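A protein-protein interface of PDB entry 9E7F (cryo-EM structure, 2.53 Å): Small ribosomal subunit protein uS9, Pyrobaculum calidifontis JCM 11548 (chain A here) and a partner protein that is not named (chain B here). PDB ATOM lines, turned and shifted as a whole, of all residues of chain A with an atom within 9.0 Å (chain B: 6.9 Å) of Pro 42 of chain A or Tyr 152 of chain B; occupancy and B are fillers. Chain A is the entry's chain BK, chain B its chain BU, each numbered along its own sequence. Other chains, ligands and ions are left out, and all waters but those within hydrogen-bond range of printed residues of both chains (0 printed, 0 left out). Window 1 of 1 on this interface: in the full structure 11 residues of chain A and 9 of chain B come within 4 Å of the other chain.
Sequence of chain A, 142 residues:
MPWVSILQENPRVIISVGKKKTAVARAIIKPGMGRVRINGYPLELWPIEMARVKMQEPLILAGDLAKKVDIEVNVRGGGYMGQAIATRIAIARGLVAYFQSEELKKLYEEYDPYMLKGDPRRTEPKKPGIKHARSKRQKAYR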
ATOM      1  N   MET A  33      18.662 -28.954  -8.498  1.00  0.00           N
ATOM      2  CA  MET A  33      17.830 -28.781  -7.319  1.00  0.00           C
ATOM      3  C   MET A  33      16.709 -27.808  -7.664  1.00  0.00           C
ATOM      4  O   MET A  33      16.488 -27.473  -8.830  1.00  0.00           O
ATOM      5  CB  MET A  33      18.651 -28.292  -6.133  1.00  0.00           C
ATOM      6  CG  MET A  33      19.801 -29.190  -5.760  1.00  0.00           C
ATOM      7  SD  MET A  33      20.789 -28.440  -4.460  1.00  0.00           S
ATOM      8  CE  MET A  33      20.632 -26.721  -4.911  1.00  0.00           C
ATOM      9  N   GLY A  34      15.997 -27.327  -6.653  1.00  0.00           N
ATOM     10  CA  GLY A  34      14.862 -26.460  -6.900  1.00  0.00           C
ATOM     11  C   GLY A  34      15.176 -24.998  -7.150  1.00  0.00           C
ATOM     12  O   GLY A  34      14.478 -24.132  -6.614  1.00  0.00           O
ATOM     13  N   ARG A  35      16.205 -24.683  -7.937  1.00  0.00           N
ATOM     14  CA  ARG A  35      16.443 -23.292  -8.304  1.00  0.00           C
ATOM     15  C   ARG A  35      15.576 -22.919  -9.492  1.00  0.00           C
ATOM     16  O   ARG A  35      15.524 -23.645 -10.487  1.00  0.00           O
ATOM     17  CB  ARG A  35      17.903 -23.024  -8.652  1.00  0.00           C
ATOM     18  CG  ARG A  35      18.921 -23.631  -7.742  1.00  0.00           C
ATOM     19  CD  ARG A  35      20.299 -23.282  -8.259  1.00  0.00           C
ATOM     20  NE  ARG A  35      20.811 -24.337  -9.121  1.00  0.00           N
ATOM     21  CZ  ARG A  35      21.569 -25.338  -8.700  1.00  0.00           C
ATOM     22  NH1 ARG A  35      21.960 -25.422  -7.440  1.00  0.00           N
ATOM     23  NH2 ARG A  35      21.953 -26.272  -9.564  1.00  0.00           N
ATOM     24  N   VAL A  36      14.905 -21.779  -9.387  1.00  0.00           N
ATOM     25  CA  VAL A  36      14.131 -21.219 -10.482  1.00  0.00           C
ATOM     26  C   VAL A  36      14.555 -19.769 -10.631  1.00  0.00           C
ATOM     27  O   VAL A  36      14.397 -18.975  -9.697  1.00  0.00           O
ATOM     28  CB  VAL A  36      12.619 -21.322 -10.235  1.00  0.00           C
ATOM     29  CG1 VAL A  36      11.864 -20.683 -11.373  1.00  0.00           C
ATOM     30  CG2 VAL A  36      12.211 -22.768 -10.060  1.00  0.00           C
ATOM     31  N   ARG A  37      15.099 -19.425 -11.790  1.00  0.00           N
ATOM     32  CA  ARG A  37      15.614 -18.088 -12.048  1.00  0.00           C
ATOM     33  C   ARG A  37      14.823 -17.482 -13.194  1.00  0.00           C
ATOM     34  O   ARG A  37      14.916 -17.950 -14.332  1.00  0.00           O
ATOM     35  CB  ARG A  37      17.103 -18.124 -12.378  1.00  0.00           C
ATOM     36  CG  ARG A  37      17.990 -18.295 -11.172  1.00  0.00           C
ATOM     37  CD  ARG A  37      19.151 -17.335 -11.233  1.00  0.00           C
ATOM     38  NE  ARG A  37      20.308 -17.839 -10.512  1.00  0.00           N
ATOM     39  CZ  ARG A  37      21.154 -17.077  -9.837  1.00  0.00           C
ATOM     40  NH1 ARG A  37      21.001 -15.766  -9.772  1.00  0.00           N
ATOM     41  NH2 ARG A  37      22.181 -17.643  -9.212  1.00  0.00           N
ATOM     42  N   ILE A  38      14.057 -16.440 -12.899  1.00  0.00           N
ATOM     43  CA  ILE A  38      13.287 -15.730 -13.907  1.00  0.00           C
ATOM     44  C   ILE A  38      14.088 -14.505 -14.310  1.00  0.00           C
ATOM     45  O   ILE A  38      14.257 -13.574 -13.514  1.00  0.00           O
ATOM     46  CB  ILE A  38      11.890 -15.352 -13.394  1.00  0.00           C
ATOM     47  CG1 ILE A  38      10.892 -16.476 -13.668  1.00  0.00           C
ATOM     48  CG2 ILE A  38      11.388 -14.115 -14.089  1.00  0.00           C
ATOM     49  CD1 ILE A  38      11.263 -17.827 -13.114  1.00  0.00           C
ATOM     50  N   ASN A  39      14.616 -14.531 -15.534  1.00  0.00           N
ATOM     51  CA  ASN A  39      15.418 -13.442 -16.081  1.00  0.00           C
ATOM     52  C   ASN A  39      16.648 -13.172 -15.224  1.00  0.00           C
ATOM     53  O   ASN A  39      17.084 -12.032 -15.064  1.00  0.00           O
ATOM     54  CB  ASN A  39      14.579 -12.184 -16.244  1.00  0.00           C
ATOM     55  CG  ASN A  39      13.924 -12.109 -17.594  1.00  0.00           C
ATOM     56  OD1 ASN A  39      13.463 -13.115 -18.122  1.00  0.00           O
ATOM     57  ND2 ASN A  39      13.889 -10.920 -18.172  1.00  0.00           N
ATOM     58  N   GLY A  40      17.208 -14.235 -14.659  1.00  0.00           N
ATOM     59  CA  GLY A  40      18.335 -14.131 -13.769  1.00  0.00           C
ATOM     60  C   GLY A  40      17.979 -13.912 -12.316  1.00  0.00           C
ATOM     61  O   GLY A  40      18.788 -14.233 -11.442  1.00  0.00           O
ATOM     62  N   TYR A  41      16.803 -13.393 -12.035  1.00  0.00           N
ATOM     63  CA  TYR A  41      16.411 -13.161 -10.654  1.00  0.00           C
ATOM     64  C   TYR A  41      15.826 -14.433 -10.070  1.00  0.00           C
ATOM     65  O   TYR A  41      15.106 -15.149 -10.771  1.00  0.00           O
ATOM     66  CB  TYR A  41      15.382 -12.047 -10.552  1.00  0.00           C
ATOM     67  CG  TYR A  41      15.831 -10.729 -11.123  1.00  0.00           C
ATOM     68  CD1 TYR A  41      15.649 -10.435 -12.460  1.00  0.00           C
ATOM     69  CD2 TYR A  41      16.439  -9.781 -10.322  1.00  0.00           C
ATOM     70  CE1 TYR A  41      16.059  -9.234 -12.986  1.00  0.00           C
ATOM     71  CE2 TYR A  41      16.854  -8.578 -10.838  1.00  0.00           C
ATOM     72  CZ  TYR A  41      16.661  -8.309 -12.173  1.00  0.00           C
ATOM     73  OH  TYR A  41      17.070  -7.107 -12.697  1.00  0.00           O
ATOM     74  N   PRO A  42      16.119 -14.758  -8.816  1.00  0.00           N
ATOM     75  CA  PRO A  42      15.456 -15.900  -8.187  1.00  0.00           C
ATOM     76  C   PRO A  42      13.970 -15.632  -8.029  1.00  0.00           C
ATOM     77  O   PRO A  42      13.542 -14.492  -7.845  1.00  0.00           O
ATOM     78  CB  PRO A  42      16.162 -16.017  -6.834  1.00  0.00           C
ATOM     79  CG  PRO A  42      17.443 -15.299  -7.010  1.00  0.00           C
ATOM     80  CD  PRO A  42      17.156 -14.183  -7.951  1.00  0.00           C
ATOM     81  N   LEU A  43      13.174 -16.697  -8.100  1.00  0.00           N
ATOM     82  CA  LEU A  43      11.729 -16.529  -8.010  1.00  0.00           C
ATOM     83  C   LEU A  43      11.291 -16.153  -6.604  1.00  0.00           C
ATOM     84  O   LEU A  43      10.201 -15.607  -6.413  1.00  0.00           O
ATOM     85  CB  LEU A  43      11.020 -17.794  -8.470  1.00  0.00           C
ATOM     86  CG  LEU A  43       9.895 -17.447  -9.433  1.00  0.00           C
ATOM     87  CD1 LEU A  43      10.330 -16.325 -10.343  1.00  0.00           C
ATOM     88  CD2 LEU A  43       9.504 -18.658 -10.236  1.00  0.00           C
ATOM     89  N   GLU A  44      12.122 -16.428  -5.607  1.00  0.00           N
ATOM     90  CA  GLU A  44      11.782 -16.075  -4.238  1.00  0.00           C
ATOM     91  C   GLU A  44      12.179 -14.632  -3.972  1.00  0.00           C
ATOM     92  O   GLU A  44      11.866 -14.076  -2.915  1.00  0.00           O
ATOM     93  CB  GLU A  44      12.443 -17.013  -3.214  1.00  0.00           C
ATOM     94  CG  GLU A  44      12.136 -18.534  -3.275  1.00  0.00           C
ATOM     95  CD  GLU A  44      12.612 -19.264  -4.519  1.00  0.00           C
ATOM     96  OE1 GLU A  44      12.838 -20.487  -4.445  1.00  0.00           O
ATOM     97  OE2 GLU A  44      12.749 -18.618  -5.575  1.00  0.00           O
ATOM     98  N   LEU A  45      12.856 -14.011  -4.934  1.00  0.00           N
ATOM     99  CA  LEU A  45      13.225 -12.609  -4.819  1.00  0.00           C
ATOM    100  C   LEU A  45      12.488 -11.739  -5.826  1.00  0.00           C
ATOM    101  O   LEU A  45      12.986 -10.660  -6.167  1.00  0.00           O
ATOM    102  CB  LEU A  45      14.730 -12.434  -4.996  1.00  0.00           C
ATOM    103  CG  LEU A  45      15.559 -12.772  -3.767  1.00  0.00           C
ATOM    104  CD1 LEU A  45      16.905 -12.126  -3.878  1.00  0.00           C
ATOM    105  CD2 LEU A  45      14.845 -12.301  -2.528  1.00  0.00           C
ATOM    106  N   TRP A  46      11.351 -12.181  -6.328  1.00  0.00           N
ATOM    107  CA  TRP A  46      10.561 -11.355  -7.223  1.00  0.00           C
ATOM    108  C   TRP A  46       9.892 -10.242  -6.428  1.00  0.00           C
ATOM    109  O   TRP A  46       9.216 -10.521  -5.432  1.00  0.00           O
ATOM    110  CB  TRP A  46       9.522 -12.206  -7.931  1.00  0.00           C
ATOM    111  CG  TRP A  46       9.013 -11.598  -9.171  1.00  0.00           C
ATOM    112  CD1 TRP A  46       7.768 -11.104  -9.384  1.00  0.00           C
ATOM    113  CD2 TRP A  46       9.734 -11.411 -10.386  1.00  0.00           C
ATOM    114  NE1 TRP A  46       7.663 -10.619 -10.657  1.00  0.00           N
ATOM    115  CE2 TRP A  46       8.861 -10.796 -11.295  1.00  0.00           C
ATOM    116  CE3 TRP A  46      11.035 -11.700 -10.793  1.00  0.00           C
ATOM    117  CZ2 TRP A  46       9.246 -10.467 -12.587  1.00  0.00           C
ATOM    118  CZ3 TRP A  46      11.410 -11.376 -12.073  1.00  0.00           C
ATOM    119  CH2 TRP A  46      10.522 -10.765 -12.954  1.00  0.00           C
ATOM    120  N   PRO A  47      10.057  -8.985  -6.820  1.00  0.00           N
ATOM    121  CA  PRO A  47       9.539  -7.879  -6.004  1.00  0.00           C
ATOM    122  C   PRO A  47       8.021  -7.795  -5.931  1.00  0.00           C
ATOM    123  O   PRO A  47       7.470  -7.633  -4.839  1.00  0.00           O
ATOM    124  CB  PRO A  47      10.134  -6.641  -6.686  1.00  0.00           C
ATOM    125  CG  PRO A  47      10.498  -7.080  -8.057  1.00  0.00           C
ATOM    126  CD  PRO A  47      10.884  -8.512  -7.941  1.00  0.00           C
ATOM    127  N   ARG A  52       4.485 -12.772  -8.314  1.00  0.00           N
ATOM    128  CA  ARG A  52       5.398 -13.822  -7.882  1.00  0.00           C
ATOM    129  C   ARG A  52       4.650 -15.099  -7.538  1.00  0.00           C
ATOM    130  O   ARG A  52       5.081 -16.199  -7.894  1.00  0.00           O
ATOM    131  CB  ARG A  52       6.215 -13.343  -6.688  1.00  0.00           C
ATOM    132  CG  ARG A  52       7.326 -14.277  -6.295  1.00  0.00           C
ATOM    133  CD  ARG A  52       7.811 -13.965  -4.907  1.00  0.00           C
ATOM    134  NE  ARG A  52       6.716 -13.957  -3.952  1.00  0.00           N
ATOM    135  CZ  ARG A  52       6.817 -13.528  -2.703  1.00  0.00           C
ATOM    136  NH1 ARG A  52       7.954 -13.050  -2.228  1.00  0.00           N
ATOM    137  NH2 ARG A  52       5.749 -13.573  -1.914  1.00  0.00           N
ATOM    138  N   MET A  55       3.499 -17.123 -10.631  1.00  0.00           N
ATOM    139  CA  MET A  55       4.541 -17.940 -11.241  1.00  0.00           C
ATOM    140  C   MET A  55       4.770 -19.217 -10.450  1.00  0.00           C
ATOM    141  O   MET A  55       4.908 -20.299 -11.026  1.00  0.00           O
ATOM    142  CB  MET A  55       5.846 -17.150 -11.334  1.00  0.00           C
ATOM    143  CG  MET A  55       5.839 -15.976 -12.284  1.00  0.00           C
ATOM    144  SD  MET A  55       7.331 -14.991 -12.058  1.00  0.00           S
ATOM    145  CE  MET A  55       7.313 -13.941 -13.505  1.00  0.00           C
ATOM    146  N   GLN A  56       4.790 -19.111  -9.127  1.00  0.00           N
ATOM    147  CA  GLN A  56       5.209 -20.210  -8.274  1.00  0.00           C
ATOM    148  C   GLN A  56       4.144 -21.278  -8.095  1.00  0.00           C
ATOM    149  O   GLN A  56       4.462 -22.346  -7.569  1.00  0.00           O
ATOM    150  CB  GLN A  56       5.617 -19.672  -6.907  1.00  0.00           C
ATOM    151  CG  GLN A  56       6.730 -18.654  -6.966  1.00  0.00           C
ATOM    152  CD  GLN A  56       7.375 -18.427  -5.625  1.00  0.00           C
ATOM    153  OE1 GLN A  56       8.576 -18.626  -5.462  1.00  0.00           O
ATOM    154  NE2 GLN A  56       6.584 -18.005  -4.653  1.00  0.00           N
ATOM    155  N   LEU A  59       4.875 -24.727  -9.245  1.00  0.00           N
ATOM    156  CA  LEU A  59       5.851 -25.365  -8.372  1.00  0.00           C
ATOM    157  C   LEU A  59       5.224 -25.782  -7.047  1.00  0.00           C
ATOM    158  O   LEU A  59       5.656 -26.763  -6.436  1.00  0.00           O
ATOM    159  CB  LEU A  59       7.025 -24.425  -8.133  1.00  0.00           C
ATOM    160  CG  LEU A  59       7.517 -23.678  -9.366  1.00  0.00           C
ATOM    161  CD1 LEU A  59       8.093 -22.344  -8.957  1.00  0.00           C
ATOM    162  CD2 LEU A  59       8.546 -24.490 -10.122  1.00  0.00           C
ATOM    163  N   VAL A  69      14.691 -30.260 -10.491  1.00  0.00           N
ATOM    164  CA  VAL A  69      14.979 -29.614 -11.766  1.00  0.00           C
ATOM    165  C   VAL A  69      15.308 -28.153 -11.526  1.00  0.00           C
ATOM    166  O   VAL A  69      14.601 -27.455 -10.797  1.00  0.00           O
ATOM    167  CB  VAL A  69      13.806 -29.735 -12.757  1.00  0.00           C
ATOM    168  CG1 VAL A  69      13.731 -31.130 -13.317  1.00  0.00           C
ATOM    169  CG2 VAL A  69      12.506 -29.356 -12.081  1.00  0.00           C
ATOM    170  N   ASP A  70      16.386 -27.695 -12.144  1.00  0.00           N
ATOM    171  CA  ASP A  70      16.654 -26.275 -12.276  1.00  0.00           C
ATOM    172  C   ASP A  70      15.778 -25.722 -13.387  1.00  0.00           C
ATOM    173  O   ASP A  70      15.541 -26.393 -14.393  1.00  0.00           O
ATOM    174  CB  ASP A  70      18.127 -26.023 -12.599  1.00  0.00           C
ATOM    175  CG  ASP A  70      19.015 -26.113 -11.378  1.00  0.00           C
ATOM    176  OD1 ASP A  70      18.637 -26.813 -10.417  1.00  0.00           O
ATOM    177  OD2 ASP A  70      20.092 -25.481 -11.380  1.00  0.00           O
ATOM    178  N   ILE A  71      15.284 -24.506 -13.198  1.00  0.00           N
ATOM    179  CA  ILE A  71      14.385 -23.884 -14.158  1.00  0.00           C
ATOM    180  C   ILE A  71      14.875 -22.472 -14.430  1.00  0.00           C
ATOM    181  O   ILE A  71      14.985 -21.662 -13.503  1.00  0.00           O
ATOM    182  CB  ILE A  71      12.934 -23.872 -13.658  1.00  0.00           C
ATOM    183  CG1 ILE A  71      12.427 -25.301 -13.515  1.00  0.00           C
ATOM    184  CG2 ILE A  71      12.049 -23.109 -14.604  1.00  0.00           C
ATOM    185  CD1 ILE A  71      11.001 -25.393 -13.091  1.00  0.00           C
ATOM    186  N   GLU A  72      15.170 -22.182 -15.689  1.00  0.00           N
ATOM    187  CA  GLU A  72      15.533 -20.846 -16.132  1.00  0.00           C
ATOM    188  C   GLU A  72      14.457 -20.356 -17.084  1.00  0.00           C
ATOM    189  O   GLU A  72      14.064 -21.079 -18.003  1.00  0.00           O
ATOM    190  CB  GLU A  72      16.895 -20.839 -16.822  1.00  0.00           C
ATOM    191  CG  GLU A  72      17.915 -21.762 -16.185  1.00  0.00           C
ATOM    192  CD  GLU A  72      18.366 -21.284 -14.822  1.00  0.00           C
ATOM    193  OE1 GLU A  72      18.683 -20.084 -14.688  1.00  0.00           O
ATOM    194  OE2 GLU A  72      18.402 -22.104 -13.882  1.00  0.00           O
ATOM    195  N   THR B   2      25.794 -13.628  -3.695  1.00  0.00           N
ATOM    196  CA  THR B   2      26.917 -13.836  -4.597  1.00  0.00           C
ATOM    197  C   THR B   2      26.949 -12.792  -5.704  1.00  0.00           C
ATOM    198  O   THR B   2      28.003 -12.249  -6.017  1.00  0.00           O
ATOM    199  CB  THR B   2      26.884 -15.242  -5.226  1.00  0.00           C
ATOM    200  OG1 THR B   2      27.817 -15.304  -6.313  1.00  0.00           O
ATOM    201  CG2 THR B   2      25.489 -15.586  -5.729  1.00  0.00           C
ATOM    202  N   SER B   3      25.793 -12.511  -6.297  1.00  0.00           N
ATOM    203  CA  SER B   3      25.700 -11.529  -7.363  1.00  0.00           C
ATOM    204  C   SER B   3      24.585 -10.550  -7.039  1.00  0.00           C
ATOM    205  O   SER B   3      23.801 -10.756  -6.112  1.00  0.00           O
ATOM    206  CB  SER B   3      25.464 -12.182  -8.727  1.00  0.00           C
ATOM    207  OG  SER B   3      25.480 -11.212  -9.757  1.00  0.00           O
ATOM    208  N   LYS B   5      21.865  -9.803  -8.527  1.00  0.00           N
ATOM    209  CA  LYS B   5      20.492 -10.244  -8.721  1.00  0.00           C
ATOM    210  C   LYS B   5      20.022 -11.223  -7.656  1.00  0.00           C
ATOM    211  O   LYS B   5      18.848 -11.600  -7.665  1.00  0.00           O
ATOM    212  CB  LYS B   5      20.330 -10.869 -10.107  1.00  0.00           C
ATOM    213  CG  LYS B   5      20.497  -9.874 -11.237  1.00  0.00           C
ATOM    214  CD  LYS B   5      20.032 -10.438 -12.563  1.00  0.00           C
ATOM    215  CE  LYS B   5      20.150  -9.395 -13.654  1.00  0.00           C
ATOM    216  NZ  LYS B   5      19.552  -9.849 -14.931  1.00  0.00           N
ATOM    217  N   ASP B   6      20.895 -11.643  -6.745  1.00  0.00           N
ATOM    218  CA  ASP B   6      20.517 -12.574  -5.692  1.00  0.00           C
ATOM    219  C   ASP B   6      20.158 -11.887  -4.384  1.00  0.00           C
ATOM    220  O   ASP B   6      19.886 -12.576  -3.400  1.00  0.00           O
ATOM    221  CB  ASP B   6      21.638 -13.588  -5.436  1.00  0.00           C
ATOM    222  CG  ASP B   6      22.364 -13.995  -6.700  1.00  0.00           C
ATOM    223  OD1 ASP B   6      21.808 -14.793  -7.484  1.00  0.00           O
ATOM    224  OD2 ASP B   6      23.504 -13.536  -6.902  1.00  0.00           O
ATOM    225  N   VAL B   7      20.150 -10.559  -4.344  1.00  0.00           N
ATOM    226  CA  VAL B   7      19.758  -9.834  -3.138  1.00  0.00           C
ATOM    227  C   VAL B   7      18.715  -8.791  -3.514  1.00  0.00           C
ATOM    228  O   VAL B   7      18.731  -8.286  -4.644  1.00  0.00           O
ATOM    229  CB  VAL B   7      20.968  -9.181  -2.458  1.00  0.00           C
ATOM    230  CG1 VAL B   7      22.023 -10.218  -2.150  1.00  0.00           C
ATOM    231  CG2 VAL B   7      21.538  -8.095  -3.338  1.00  0.00           C
ATOM    232  N   GLU B 148      15.308 -20.464   2.105  1.00  0.00           N
ATOM    233  CA  GLU B 148      15.005 -20.886   0.744  1.00  0.00           C
ATOM    234  C   GLU B 148      15.929 -20.238  -0.275  1.00  0.00           C
ATOM    235  O   GLU B 148      16.029 -20.730  -1.402  1.00  0.00           O
ATOM    236  CB  GLU B 148      13.539 -20.588   0.347  1.00  0.00           C
ATOM    237  CG  GLU B 148      12.314 -21.013   1.249  1.00  0.00           C
ATOM    238  CD  GLU B 148      12.329 -20.579   2.713  1.00  0.00           C
ATOM    239  OE1 GLU B 148      12.218 -19.366   2.984  1.00  0.00           O
ATOM    240  OE2 GLU B 148      12.481 -21.457   3.589  1.00  0.00           O
ATOM    241  N   LEU B 149      16.598 -19.150   0.087  1.00  0.00           N
ATOM    242  CA  LEU B 149      17.597 -18.530  -0.767  1.00  0.00           C
ATOM    243  C   LEU B 149      18.953 -19.206  -0.660  1.00  0.00           C
ATOM    244  O   LEU B 149      19.903 -18.770  -1.318  1.00  0.00           O
ATOM    245  CB  LEU B 149      17.739 -17.050  -0.419  1.00  0.00           C
ATOM    246  CG  LEU B 149      16.438 -16.286  -0.196  1.00  0.00           C
ATOM    247  CD1 LEU B 149      16.717 -14.812  -0.015  1.00  0.00           C
ATOM    248  CD2 LEU B 149      15.500 -16.511  -1.366  1.00  0.00           C
ATOM    249  N   ALA B 150      19.071 -20.249   0.161  1.00  0.00           N
ATOM    250  CA  ALA B 150      20.361 -20.901   0.346  1.00  0.00           C
ATOM    251  C   ALA B 150      20.814 -21.609  -0.920  1.00  0.00           C
ATOM    252  O   ALA B 150      22.016 -21.737  -1.167  1.00  0.00           O
ATOM    253  CB  ALA B 150      20.288 -21.882   1.513  1.00  0.00           C
ATOM    254  N   LYS B 151      19.871 -22.070  -1.744  1.00  0.00           N
ATOM    255  CA  LYS B 151      20.246 -22.795  -2.954  1.00  0.00           C
ATOM    256  C   LYS B 151      20.753 -21.877  -4.056  1.00  0.00           C
ATOM    257  O   LYS B 151      21.232 -22.368  -5.081  1.00  0.00           O
ATOM    258  CB  LYS B 151      19.065 -23.608  -3.477  1.00  0.00           C
ATOM    259  CG  LYS B 151      17.917 -22.776  -3.994  1.00  0.00           C
ATOM    260  CD  LYS B 151      16.643 -23.587  -4.037  1.00  0.00           C
ATOM    261  CE  LYS B 151      16.099 -23.822  -2.631  1.00  0.00           C
ATOM    262  NZ  LYS B 151      14.643 -23.531  -2.535  1.00  0.00           N
ATOM    263  N   TYR B 152      20.639 -20.565  -3.886  1.00  0.00           N
ATOM    264  CA  TYR B 152      21.073 -19.631  -4.913  1.00  0.00           C
ATOM    265  C   TYR B 152      22.455 -19.064  -4.642  1.00  0.00           C
ATOM    266  O   TYR B 152      23.116 -18.593  -5.574  1.00  0.00           O
ATOM    267  CB  TYR B 152      20.071 -18.482  -5.041  1.00  0.00           C
ATOM    268  CG  TYR B 152      18.674 -18.921  -5.401  1.00  0.00           C
ATOM    269  CD1 TYR B 152      17.753 -19.248  -4.418  1.00  0.00           C
ATOM    270  CD2 TYR B 152      18.272 -18.999  -6.723  1.00  0.00           C
ATOM    271  CE1 TYR B 152      16.480 -19.648  -4.741  1.00  0.00           C
ATOM    272  CE2 TYR B 152      16.999 -19.397  -7.054  1.00  0.00           C
ATOM    273  CZ  TYR B 152      16.107 -19.720  -6.059  1.00  0.00           C
ATOM    274  OH  TYR B 152      14.836 -20.116  -6.384  1.00  0.00           O
ATOM    275  N   VAL B 153      22.907 -19.092  -3.391  1.00  0.00           N
ATOM    276  CA  VAL B 153      24.190 -18.499  -3.041  1.00  0.00           C
ATOM    277  C   VAL B 153      25.109 -19.556  -2.447  1.00  0.00           C
ATOM    278  O   VAL B 153      26.336 -19.462  -2.564  1.00  0.00           O
ATOM    279  CB  VAL B 153      24.002 -17.324  -2.070  1.00  0.00           C
ATOM    280  CG1 VAL B 153      23.891 -16.031  -2.835  1.00  0.00           C
ATOM    281  CG2 VAL B 153      22.762 -17.541  -1.224  1.00  0.00           C
ATOM    282  N   ALA B 154      24.527 -20.570  -1.813  1.00  0.00           N
ATOM    283  CA  ALA B 154      25.283 -21.621  -1.135  1.00  0.00           C
ATOM    284  C   ALA B 154      24.731 -22.984  -1.526  1.00  0.00           C
ATOM    285  O   ALA B 154      24.074 -23.655  -0.721  1.00  0.00           O
ATOM    286  CB  ALA B 154      25.239 -21.431   0.382  1.00  0.00           C
ATOM    287  N   PRO B 155      24.975 -23.422  -2.758  1.00  0.00           N
ATOM    288  CA  PRO B 155      24.435 -24.703  -3.221  1.00  0.00           C
ATOM    289  C   PRO B 155      25.038 -25.866  -2.457  1.00  0.00           C
ATOM    290  O   PRO B 155      26.259 -25.921  -2.250  1.00  0.00           O
ATOM    291  CB  PRO B 155      24.841 -24.743  -4.702  1.00  0.00           C
ATOM    292  CG  PRO B 155      25.126 -23.328  -5.063  1.00  0.00           C
ATOM    293  CD  PRO B 155      25.688 -22.708  -3.828  1.00  0.00           C
ATOM    294  N   PRO B 156      24.208 -26.813  -2.004  1.00  0.00           N
ATOM    295  CA  PRO B 156      24.632 -28.016  -1.281  1.00  0.00           C
ATOM    296  C   PRO B 156      25.467 -28.956  -2.143  1.00  0.00           C
ATOM    297  O   PRO B 156      25.258 -28.984  -3.354  1.00  0.00           O
ATOM    298  CB  PRO B 156      23.303 -28.675  -0.892  1.00  0.00           C
ATOM    299  CG  PRO B 156      22.307 -27.575  -0.931  1.00  0.00           C
ATOM    300  CD  PRO B 156      22.741 -26.711  -2.067  1.00  0.00           C
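O of Asn 39 of chain A is in hydrogen-bond range of NZ of Lys 5 of chain B (3.3 Å).
The side-chain carboxylate (OE2) of Glu 44 of chain A is in hydrogen-bond range of the side-chain hydroxyl (OH) of Tyr 152 of chain B.
NH1 of Arg 37 of chain A is in salt-bridge range of OD1 of Asp 6 of chain B, 2.6 Å away.
The backbone NH (N) of Val 36 of chain A sits at hydrogen-bond distance from the side-chain hydroxyl (OH) of Tyr 152 of chain B, 3.4 Å away.
The backbone carbonyl oxygen (O) of Ile 71 of chain A is in hydrogen-bond range of the backbone NH (N) of Arg 37 of chain A, at 2.8 Å.
NE of Arg 35 of chain A is in salt-bridge range of OD2 of Asp 70 of chain A (2.6 Å).
O of Arg 35 of chain A sits at hydrogen-bond distance from N of Ile 71 of chain A, at 2.9 Å.
OD1 of Asp 70 of chain A is in hydrogen-bond range of N of Met 33 of chain A (2.9 Å).
The backbone NH (N) of Leu 43 of chain A sits at hydrogen-bond distance from the backbone carbonyl oxygen (O) of Val 36 of chain A, 3.0 Å away.
NH1 of Arg 37 of chain A sits close to O of Gly 40 of chain A.
Met 33 of chain A touches Lys 151 of chain B.
Met 33 of chain A touches Pro 156 of chain B (SD to CD, 3.5 Å).
Gly 34 of chain A touches Lys 151 of chain B (O to CD, 3.4 Å).
Arg 35 of chain A touches Lys 151 of chain B.
Tyr 152 of chain B touches Arg 37 of chain A.
Lys 5 of chain B touches Gly 40 of chain A.
Lys 5 of chain B touches Tyr 41 of chain A.
Pro 42 of chain A touches Lys 5 of chain B.
Pro 42 of chain A touches Tyr 152 of chain B.
Leu 45 of chain A touches Asp 6 of chain B (CD1 to O, 3.1 Å).
Of chain B, only Lys 5 (3.1 Å) and Tyr 152 (3.5 Å) come within 4 Å of Pro 42 of chain A.
Printed residues of chain A within 4 Å of Lys 5 of chain B: Asn 39 (3.3 Å), Gly 40 (3.9 Å), Tyr 41 (3.9 Å) and Pro 42 (3.1 Å).
Of the printed residues of chain B, Tyr 41 of chain A touches Lys 5.
Of the printed residues of chain B, Glu 44 of chain A touches Leu 149 (3.6 Å) and Tyr 152 (2.7 Å).
Pro 155 of chain B touches none of the printed residues of chain A.
Glu 72 of chain A touches none of the printed residues of chain B.
The nearest printed residue of chain A that does not touch Tyr 152 of chain B is Gly 34 of chain A (4.04 Å).
Of the 14 printed residues of chain B, 7 touch a printed residue of chain A.
Of the 23 printed residues of chain A, 11 touch a printed residue of chain B.
Hydrophobic or aromatic side chains of chain A within 4 Å of the printed part of chain B: Met 33, Tyr 41, Pro 42 and Leu 45.
Among the printed residues, 16 pairs touch across the chains.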
